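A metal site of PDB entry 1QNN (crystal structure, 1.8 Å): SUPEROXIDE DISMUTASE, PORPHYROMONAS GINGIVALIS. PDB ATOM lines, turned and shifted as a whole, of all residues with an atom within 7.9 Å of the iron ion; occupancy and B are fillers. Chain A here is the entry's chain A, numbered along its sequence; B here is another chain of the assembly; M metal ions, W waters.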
ATOM      1  N   HIS A  27       9.390  22.315  -5.972  1.00  0.00           N
ATOM      2  CA  HIS A  27       8.815  23.492  -5.329  1.00  0.00           C
ATOM      3  C   HIS A  27       9.841  24.601  -5.083  1.00  0.00           C
ATOM      4  O   HIS A  27       9.613  25.771  -5.423  1.00  0.00           O
ATOM      5  CB  HIS A  27       8.154  23.089  -4.013  1.00  0.00           C
ATOM      6  CG  HIS A  27       7.031  23.979  -3.615  1.00  0.00           C
ATOM      7  ND1 HIS A  27       6.189  23.700  -2.562  1.00  0.00           N
ATOM      8  CD2 HIS A  27       6.618  25.168  -4.110  1.00  0.00           C
ATOM      9  CE1 HIS A  27       5.310  24.685  -2.431  1.00  0.00           C
ATOM     10  NE2 HIS A  27       5.557  25.577  -3.358  1.00  0.00           N
ATOM     11  N   HIS A  28      10.964  24.228  -4.488  1.00  0.00           N
ATOM     12  CA  HIS A  28      12.018  25.181  -4.204  1.00  0.00           C
ATOM     13  C   HIS A  28      12.889  25.455  -5.431  1.00  0.00           C
ATOM     14  O   HIS A  28      13.023  26.604  -5.856  1.00  0.00           O
ATOM     15  CB  HIS A  28      12.899  24.686  -3.056  1.00  0.00           C
ATOM     16  CG  HIS A  28      14.016  25.618  -2.710  1.00  0.00           C
ATOM     17  ND1 HIS A  28      15.248  25.558  -3.319  1.00  0.00           N
ATOM     18  CD2 HIS A  28      14.063  26.685  -1.866  1.00  0.00           C
ATOM     19  CE1 HIS A  28      16.009  26.553  -2.877  1.00  0.00           C
ATOM     20  NE2 HIS A  28      15.311  27.251  -1.992  1.00  0.00           N
ATOM     21  N   HIS A  31       9.846  26.019  -9.058  1.00  0.00           N
ATOM     22  CA  HIS A  31       8.828  27.034  -8.877  1.00  0.00           C
ATOM     23  C   HIS A  31       9.382  28.314  -8.258  1.00  0.00           C
ATOM     24  O   HIS A  31       9.317  29.383  -8.870  1.00  0.00           O
ATOM     25  CB  HIS A  31       7.689  26.485  -7.997  1.00  0.00           C
ATOM     26  CG  HIS A  31       6.865  25.426  -8.668  1.00  0.00           C
ATOM     27  ND1 HIS A  31       5.883  25.715  -9.589  1.00  0.00           N
ATOM     28  CD2 HIS A  31       6.891  24.078  -8.552  1.00  0.00           C
ATOM     29  CE1 HIS A  31       5.330  24.594 -10.003  1.00  0.00           C
ATOM     30  NE2 HIS A  31       5.922  23.587  -9.393  1.00  0.00           N
ATOM     31  N   LEU A  32       9.933  28.220  -7.054  1.00  0.00           N
ATOM     32  CA  LEU A  32      10.460  29.415  -6.405  1.00  0.00           C
ATOM     33  C   LEU A  32      11.554  30.075  -7.230  1.00  0.00           C
ATOM     34  O   LEU A  32      11.561  31.295  -7.391  1.00  0.00           O
ATOM     35  CB  LEU A  32      10.995  29.072  -5.022  1.00  0.00           C
ATOM     36  CG  LEU A  32      11.433  30.252  -4.181  1.00  0.00           C
ATOM     37  CD1 LEU A  32      10.413  31.422  -4.310  1.00  0.00           C
ATOM     38  CD2 LEU A  32      11.585  29.797  -2.742  1.00  0.00           C
ATOM     39  N   TYR A  35       9.980  32.250  -9.767  1.00  0.00           N
ATOM     40  CA  TYR A  35       9.371  33.469  -9.247  1.00  0.00           C
ATOM     41  C   TYR A  35      10.455  34.516  -8.950  1.00  0.00           C
ATOM     42  O   TYR A  35      10.262  35.706  -9.186  1.00  0.00           O
ATOM     43  CB  TYR A  35       8.582  33.161  -7.967  1.00  0.00           C
ATOM     44  CG  TYR A  35       7.337  32.312  -8.179  1.00  0.00           C
ATOM     45  CD1 TYR A  35       6.473  32.562  -9.241  1.00  0.00           C
ATOM     46  CD2 TYR A  35       7.021  31.266  -7.305  1.00  0.00           C
ATOM     47  CE1 TYR A  35       5.310  31.807  -9.424  1.00  0.00           C
ATOM     48  CE2 TYR A  35       5.864  30.498  -7.490  1.00  0.00           C
ATOM     49  CZ  TYR A  35       5.018  30.788  -8.547  1.00  0.00           C
ATOM     50  OH  TYR A  35       3.855  30.070  -8.711  1.00  0.00           O
ATOM     51  N   GLN A  70       4.587  35.644  -4.410  1.00  0.00           N
ATOM     52  CA  GLN A  70       4.958  34.247  -4.366  1.00  0.00           C
ATOM     53  C   GLN A  70       6.362  34.069  -3.779  1.00  0.00           C
ATOM     54  O   GLN A  70       6.638  33.083  -3.084  1.00  0.00           O
ATOM     55  CB  GLN A  70       4.880  33.640  -5.770  1.00  0.00           C
ATOM     56  CG  GLN A  70       3.465  33.295  -6.211  1.00  0.00           C
ATOM     57  CD  GLN A  70       2.853  32.179  -5.385  1.00  0.00           C
ATOM     58  OE1 GLN A  70       2.528  32.371  -4.223  1.00  0.00           O
ATOM     59  NE2 GLN A  70       2.689  31.000  -5.989  1.00  0.00           N
ATOM     60  N   ASN A  73       5.921  34.665  -0.050  1.00  0.00           N
ATOM     61  CA  ASN A  73       5.148  33.534   0.455  1.00  0.00           C
ATOM     62  C   ASN A  73       6.018  32.290   0.689  1.00  0.00           C
ATOM     63  O   ASN A  73       6.047  31.745   1.791  1.00  0.00           O
ATOM     64  CB  ASN A  73       4.005  33.217  -0.520  1.00  0.00           C
ATOM     65  CG  ASN A  73       2.775  34.076  -0.272  1.00  0.00           C
ATOM     66  OD1 ASN A  73       2.500  34.471   0.857  1.00  0.00           O
ATOM     67  ND2 ASN A  73       2.013  34.354  -1.326  1.00  0.00           N
ATOM     68  N   HIS A  74       6.729  31.856  -0.344  1.00  0.00           N
ATOM     69  CA  HIS A  74       7.580  30.673  -0.252  1.00  0.00           C
ATOM     70  C   HIS A  74       8.787  30.830   0.678  1.00  0.00           C
ATOM     71  O   HIS A  74       9.220  29.866   1.309  1.00  0.00           O
ATOM     72  CB  HIS A  74       8.058  30.274  -1.633  1.00  0.00           C
ATOM     73  CG  HIS A  74       6.976  29.687  -2.484  1.00  0.00           C
ATOM     74  ND1 HIS A  74       6.139  30.464  -3.257  1.00  0.00           N
ATOM     75  CD2 HIS A  74       6.559  28.406  -2.655  1.00  0.00           C
ATOM     76  CE1 HIS A  74       5.259  29.687  -3.867  1.00  0.00           C
ATOM     77  NE2 HIS A  74       5.497  28.448  -3.519  1.00  0.00           N
ATOM     78  N   TYR A  77       7.301  30.251   3.856  1.00  0.00           N
ATOM     79  CA  TYR A  77       6.804  28.874   3.868  1.00  0.00           C
ATOM     80  C   TYR A  77       7.914  27.871   4.155  1.00  0.00           C
ATOM     81  O   TYR A  77       7.830  27.078   5.084  1.00  0.00           O
ATOM     82  CB  TYR A  77       6.163  28.565   2.513  1.00  0.00           C
ATOM     83  CG  TYR A  77       5.659  27.151   2.303  1.00  0.00           C
ATOM     84  CD1 TYR A  77       4.443  26.724   2.841  1.00  0.00           C
ATOM     85  CD2 TYR A  77       6.347  26.269   1.459  1.00  0.00           C
ATOM     86  CE1 TYR A  77       3.919  25.461   2.558  1.00  0.00           C
ATOM     87  CE2 TYR A  77       5.836  25.006   1.171  1.00  0.00           C
ATOM     88  CZ  TYR A  77       4.626  24.608   1.700  1.00  0.00           C
ATOM     89  OH  TYR A  77       4.098  23.389   1.351  1.00  0.00           O
ATOM     90  N   PHE A  78       8.976  27.939   3.367  1.00  0.00           N
ATOM     91  CA  PHE A  78      10.097  27.014   3.511  1.00  0.00           C
ATOM     92  C   PHE A  78      10.866  27.125   4.813  1.00  0.00           C
ATOM     93  O   PHE A  78      11.387  26.130   5.302  1.00  0.00           O
ATOM     94  CB  PHE A  78      11.056  27.168   2.335  1.00  0.00           C
ATOM     95  CG  PHE A  78      10.527  26.568   1.059  1.00  0.00           C
ATOM     96  CD1 PHE A  78      10.473  27.325  -0.113  1.00  0.00           C
ATOM     97  CD2 PHE A  78      10.067  25.268   1.030  1.00  0.00           C
ATOM     98  CE1 PHE A  78       9.959  26.782  -1.278  1.00  0.00           C
ATOM     99  CE2 PHE A  78       9.543  24.721  -0.142  1.00  0.00           C
ATOM    100  CZ  PHE A  78       9.498  25.486  -1.293  1.00  0.00           C
ATOM    101  N   GLY A 122      -3.875  29.118  -4.017  1.00  0.00           N
ATOM    102  CA  GLY A 122      -3.826  30.169  -3.018  1.00  0.00           C
ATOM    103  C   GLY A 122      -3.059  29.807  -1.779  1.00  0.00           C
ATOM    104  O   GLY A 122      -2.340  28.792  -1.738  1.00  0.00           O
ATOM    105  N   TRP A 123      -3.258  30.608  -0.741  1.00  0.00           N
ATOM    106  CA  TRP A 123      -2.561  30.431   0.526  1.00  0.00           C
ATOM    107  C   TRP A 123      -3.509  30.684   1.674  1.00  0.00           C
ATOM    108  O   TRP A 123      -4.414  31.505   1.559  1.00  0.00           O
ATOM    109  CB  TRP A 123      -1.418  31.452   0.631  1.00  0.00           C
ATOM    110  CG  TRP A 123      -0.277  31.204  -0.309  1.00  0.00           C
ATOM    111  CD1 TRP A 123      -0.222  31.510  -1.646  1.00  0.00           C
ATOM    112  CD2 TRP A 123       0.966  30.571   0.012  1.00  0.00           C
ATOM    113  NE1 TRP A 123       0.979  31.108  -2.168  1.00  0.00           N
ATOM    114  CE2 TRP A 123       1.728  30.529  -1.172  1.00  0.00           C
ATOM    115  CE3 TRP A 123       1.506  30.032   1.187  1.00  0.00           C
ATOM    116  CZ2 TRP A 123       3.010  29.971  -1.228  1.00  0.00           C
ATOM    117  CZ3 TRP A 123       2.785  29.479   1.144  1.00  0.00           C
ATOM    118  CH2 TRP A 123       3.517  29.457  -0.059  1.00  0.00           C
ATOM    119  N   ASN A 141      -4.307  32.820  -5.027  1.00  0.00           N
ATOM    120  CA  ASN A 141      -3.100  32.911  -5.836  1.00  0.00           C
ATOM    121  C   ASN A 141      -1.829  33.344  -5.131  1.00  0.00           C
ATOM    122  O   ASN A 141      -1.277  32.592  -4.330  1.00  0.00           O
ATOM    123  CB  ASN A 141      -3.393  33.790  -7.055  1.00  0.00           C
ATOM    124  CG  ASN A 141      -4.486  33.187  -7.933  1.00  0.00           C
ATOM    125  OD1 ASN A 141      -4.677  31.985  -7.927  1.00  0.00           O
ATOM    126  ND2 ASN A 141      -5.187  34.027  -8.673  1.00  0.00           N
ATOM    127  N   PHE A 156       0.186  28.227   4.780  1.00  0.00           N
ATOM    128  CA  PHE A 156       0.124  26.899   4.172  1.00  0.00           C
ATOM    129  C   PHE A 156      -0.169  27.112   2.696  1.00  0.00           C
ATOM    130  O   PHE A 156      -1.097  27.826   2.341  1.00  0.00           O
ATOM    131  CB  PHE A 156      -0.997  26.064   4.807  1.00  0.00           C
ATOM    132  CG  PHE A 156      -0.627  25.437   6.132  1.00  0.00           C
ATOM    133  CD1 PHE A 156       0.635  25.637   6.691  1.00  0.00           C
ATOM    134  CD2 PHE A 156      -1.553  24.664   6.831  1.00  0.00           C
ATOM    135  CE1 PHE A 156       0.971  25.064   7.911  1.00  0.00           C
ATOM    136  CE2 PHE A 156      -1.221  24.087   8.060  1.00  0.00           C
ATOM    137  CZ  PHE A 156       0.047  24.287   8.597  1.00  0.00           C
ATOM    138  N   ASP A 157       0.632  26.502   1.837  1.00  0.00           N
ATOM    139  CA  ASP A 157       0.471  26.623   0.388  1.00  0.00           C
ATOM    140  C   ASP A 157      -0.566  25.611  -0.114  1.00  0.00           C
ATOM    141  O   ASP A 157      -0.407  24.409   0.097  1.00  0.00           O
ATOM    142  CB  ASP A 157       1.843  26.381  -0.284  1.00  0.00           C
ATOM    143  CG  ASP A 157       1.857  26.667  -1.778  1.00  0.00           C
ATOM    144  OD1 ASP A 157       0.799  27.027  -2.344  1.00  0.00           O
ATOM    145  OD2 ASP A 157       2.942  26.552  -2.408  1.00  0.00           O
ATOM    146  N   VAL A 158      -1.655  26.082  -0.742  1.00  0.00           N
ATOM    147  CA  VAL A 158      -2.639  25.143  -1.266  1.00  0.00           C
ATOM    148  C   VAL A 158      -2.652  25.091  -2.795  1.00  0.00           C
ATOM    149  O   VAL A 158      -3.595  24.600  -3.422  1.00  0.00           O
ATOM    150  CB  VAL A 158      -4.065  25.390  -0.709  1.00  0.00           C
ATOM    151  CG1 VAL A 158      -4.047  25.218   0.823  1.00  0.00           C
ATOM    152  CG2 VAL A 158      -4.562  26.792  -1.082  1.00  0.00           C
ATOM    153  N   TRP A 159      -1.594  25.621  -3.405  1.00  0.00           N
ATOM    154  CA  TRP A 159      -1.462  25.513  -4.856  1.00  0.00           C
ATOM    155  C   TRP A 159      -1.208  24.003  -4.945  1.00  0.00           C
ATOM    156  O   TRP A 159      -0.485  23.460  -4.107  1.00  0.00           O
ATOM    157  CB  TRP A 159      -0.212  26.225  -5.357  1.00  0.00           C
ATOM    158  CG  TRP A 159      -0.368  27.684  -5.588  1.00  0.00           C
ATOM    159  CD1 TRP A 159      -0.696  28.634  -4.648  1.00  0.00           C
ATOM    160  CD2 TRP A 159      -0.196  28.368  -6.822  1.00  0.00           C
ATOM    161  NE1 TRP A 159      -0.739  29.875  -5.250  1.00  0.00           N
ATOM    162  CE2 TRP A 159      -0.439  29.744  -6.569  1.00  0.00           C
ATOM    163  CE3 TRP A 159       0.124  27.960  -8.120  1.00  0.00           C
ATOM    164  CZ2 TRP A 159      -0.359  30.708  -7.590  1.00  0.00           C
ATOM    165  CZ3 TRP A 159       0.210  28.924  -9.124  1.00  0.00           C
ATOM    166  CH2 TRP A 159      -0.037  30.284  -8.845  1.00  0.00           C
ATOM    167  N   GLU A 160      -1.787  23.322  -5.927  1.00  0.00           N
ATOM    168  CA  GLU A 160      -1.596  21.882  -6.041  1.00  0.00           C
ATOM    169  C   GLU A 160      -0.154  21.392  -6.137  1.00  0.00           C
ATOM    170  O   GLU A 160       0.120  20.258  -5.741  1.00  0.00           O
ATOM    171  CB  GLU A 160      -2.408  21.351  -7.226  1.00  0.00           C
ATOM    172  CG  GLU A 160      -3.914  21.512  -7.030  1.00  0.00           C
ATOM    173  CD  GLU A 160      -4.724  21.104  -8.253  1.00  0.00           C
ATOM    174  OE1 GLU A 160      -4.384  21.512  -9.382  1.00  0.00           O
ATOM    175  OE2 GLU A 160      -5.713  20.363  -8.083  1.00  0.00           O
ATOM    176  N   HIS A 161       0.764  22.194  -6.652  1.00  0.00           N
ATOM    177  CA  HIS A 161       2.161  21.729  -6.749  1.00  0.00           C
ATOM    178  C   HIS A 161       2.774  21.487  -5.385  1.00  0.00           C
ATOM    179  O   HIS A 161       3.790  20.803  -5.265  1.00  0.00           O
ATOM    180  CB  HIS A 161       3.029  22.739  -7.524  1.00  0.00           C
ATOM    181  CG  HIS A 161       3.130  24.091  -6.894  1.00  0.00           C
ATOM    182  ND1 HIS A 161       2.868  25.252  -7.582  1.00  0.00           N
ATOM    183  CD2 HIS A 161       3.489  24.469  -5.636  1.00  0.00           C
ATOM    184  CE1 HIS A 161       3.054  26.289  -6.788  1.00  0.00           C
ATOM    185  NE2 HIS A 161       3.438  25.838  -5.605  1.00  0.00           N
ATOM    186  N   ALA A 162       2.157  22.042  -4.353  1.00  0.00           N
ATOM    187  CA  ALA A 162       2.682  21.871  -3.002  1.00  0.00           C
ATOM    188  C   ALA A 162       2.529  20.470  -2.464  1.00  0.00           C
ATOM    189  O   ALA A 162       3.315  20.044  -1.607  1.00  0.00           O
ATOM    190  CB  ALA A 162       2.003  22.834  -2.062  1.00  0.00           C
ATOM    191  N   TYR A 163       1.526  19.744  -2.968  1.00  0.00           N
ATOM    192  CA  TYR A 163       1.223  18.418  -2.462  1.00  0.00           C
ATOM    193  C   TYR A 163       0.848  17.355  -3.472  1.00  0.00           C
ATOM    194  O   TYR A 163       0.664  16.203  -3.076  1.00  0.00           O
ATOM    195  CB  TYR A 163       0.087  18.494  -1.468  1.00  0.00           C
ATOM    196  CG  TYR A 163      -1.190  19.103  -2.056  1.00  0.00           C
ATOM    197  CD1 TYR A 163      -2.073  18.333  -2.827  1.00  0.00           C
ATOM    198  CD2 TYR A 163      -1.503  20.451  -1.843  1.00  0.00           C
ATOM    199  CE1 TYR A 163      -3.233  18.879  -3.369  1.00  0.00           C
ATOM    200  CE2 TYR A 163      -2.662  21.021  -2.385  1.00  0.00           C
ATOM    201  CZ  TYR A 163      -3.526  20.227  -3.145  1.00  0.00           C
ATOM    202  OH  TYR A 163      -4.655  20.789  -3.687  1.00  0.00           O
ATOM    203  N   GLU B 160      -3.000  22.804 -12.124  1.00  0.00           N
ATOM    204  CA  GLU B 160      -1.801  21.979 -12.073  1.00  0.00           C
ATOM    205  C   GLU B 160      -2.062  20.472 -12.096  1.00  0.00           C
ATOM    206  O   GLU B 160      -1.241  19.711 -12.620  1.00  0.00           O
ATOM    207  CB  GLU B 160      -0.960  22.378 -10.850  1.00  0.00           C
ATOM    208  CG  GLU B 160      -0.184  23.669 -11.112  1.00  0.00           C
ATOM    209  CD  GLU B 160       0.541  24.205  -9.897  1.00  0.00           C
ATOM    210  OE1 GLU B 160       0.002  24.093  -8.780  1.00  0.00           O
ATOM    211  OE2 GLU B 160       1.644  24.749 -10.077  1.00  0.00           O
HETATM  212 FE    FE M   1       4.007  26.965  -3.895  1.00  0.00          FE
HETATM  213  O   HOH W   1       2.610  28.474  -4.325  1.00  0.00           O
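The side-chain carboxylate of Asp 157 is in hydrogen-bond range of the backbone NH of Trp 159. A ring nitrogen (ND1) of His 161 sits at hydrogen-bond distance from the side-chain carboxylate (OE2) of Glu 160 of chain B (2.8 Å). O of Gln 70 sits at hydrogen-bond distance from ND1 of His 74 (2.7 Å). O of His 27 lies within hydrogen-bond range of N of Leu 32 (3.0 Å).
Four residues have an atom within 4 Å of the iron ion: His 27, His 74, Asp 157 and His 161. Along chain A the residues within 4 Å of the iron ion span positions 27 to 161.
The iron ion is bound by OD2 of Asp 157, water W1, NE2 of His 161, NE2 of His 74 and NE2 of His 27.
Water W1 bridges the side-chain amide nitrogen (NE2) of Gln 70 (3.0 Å) and the side-chain carboxylate (OD1) of Asp 157 (3.0 Å).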
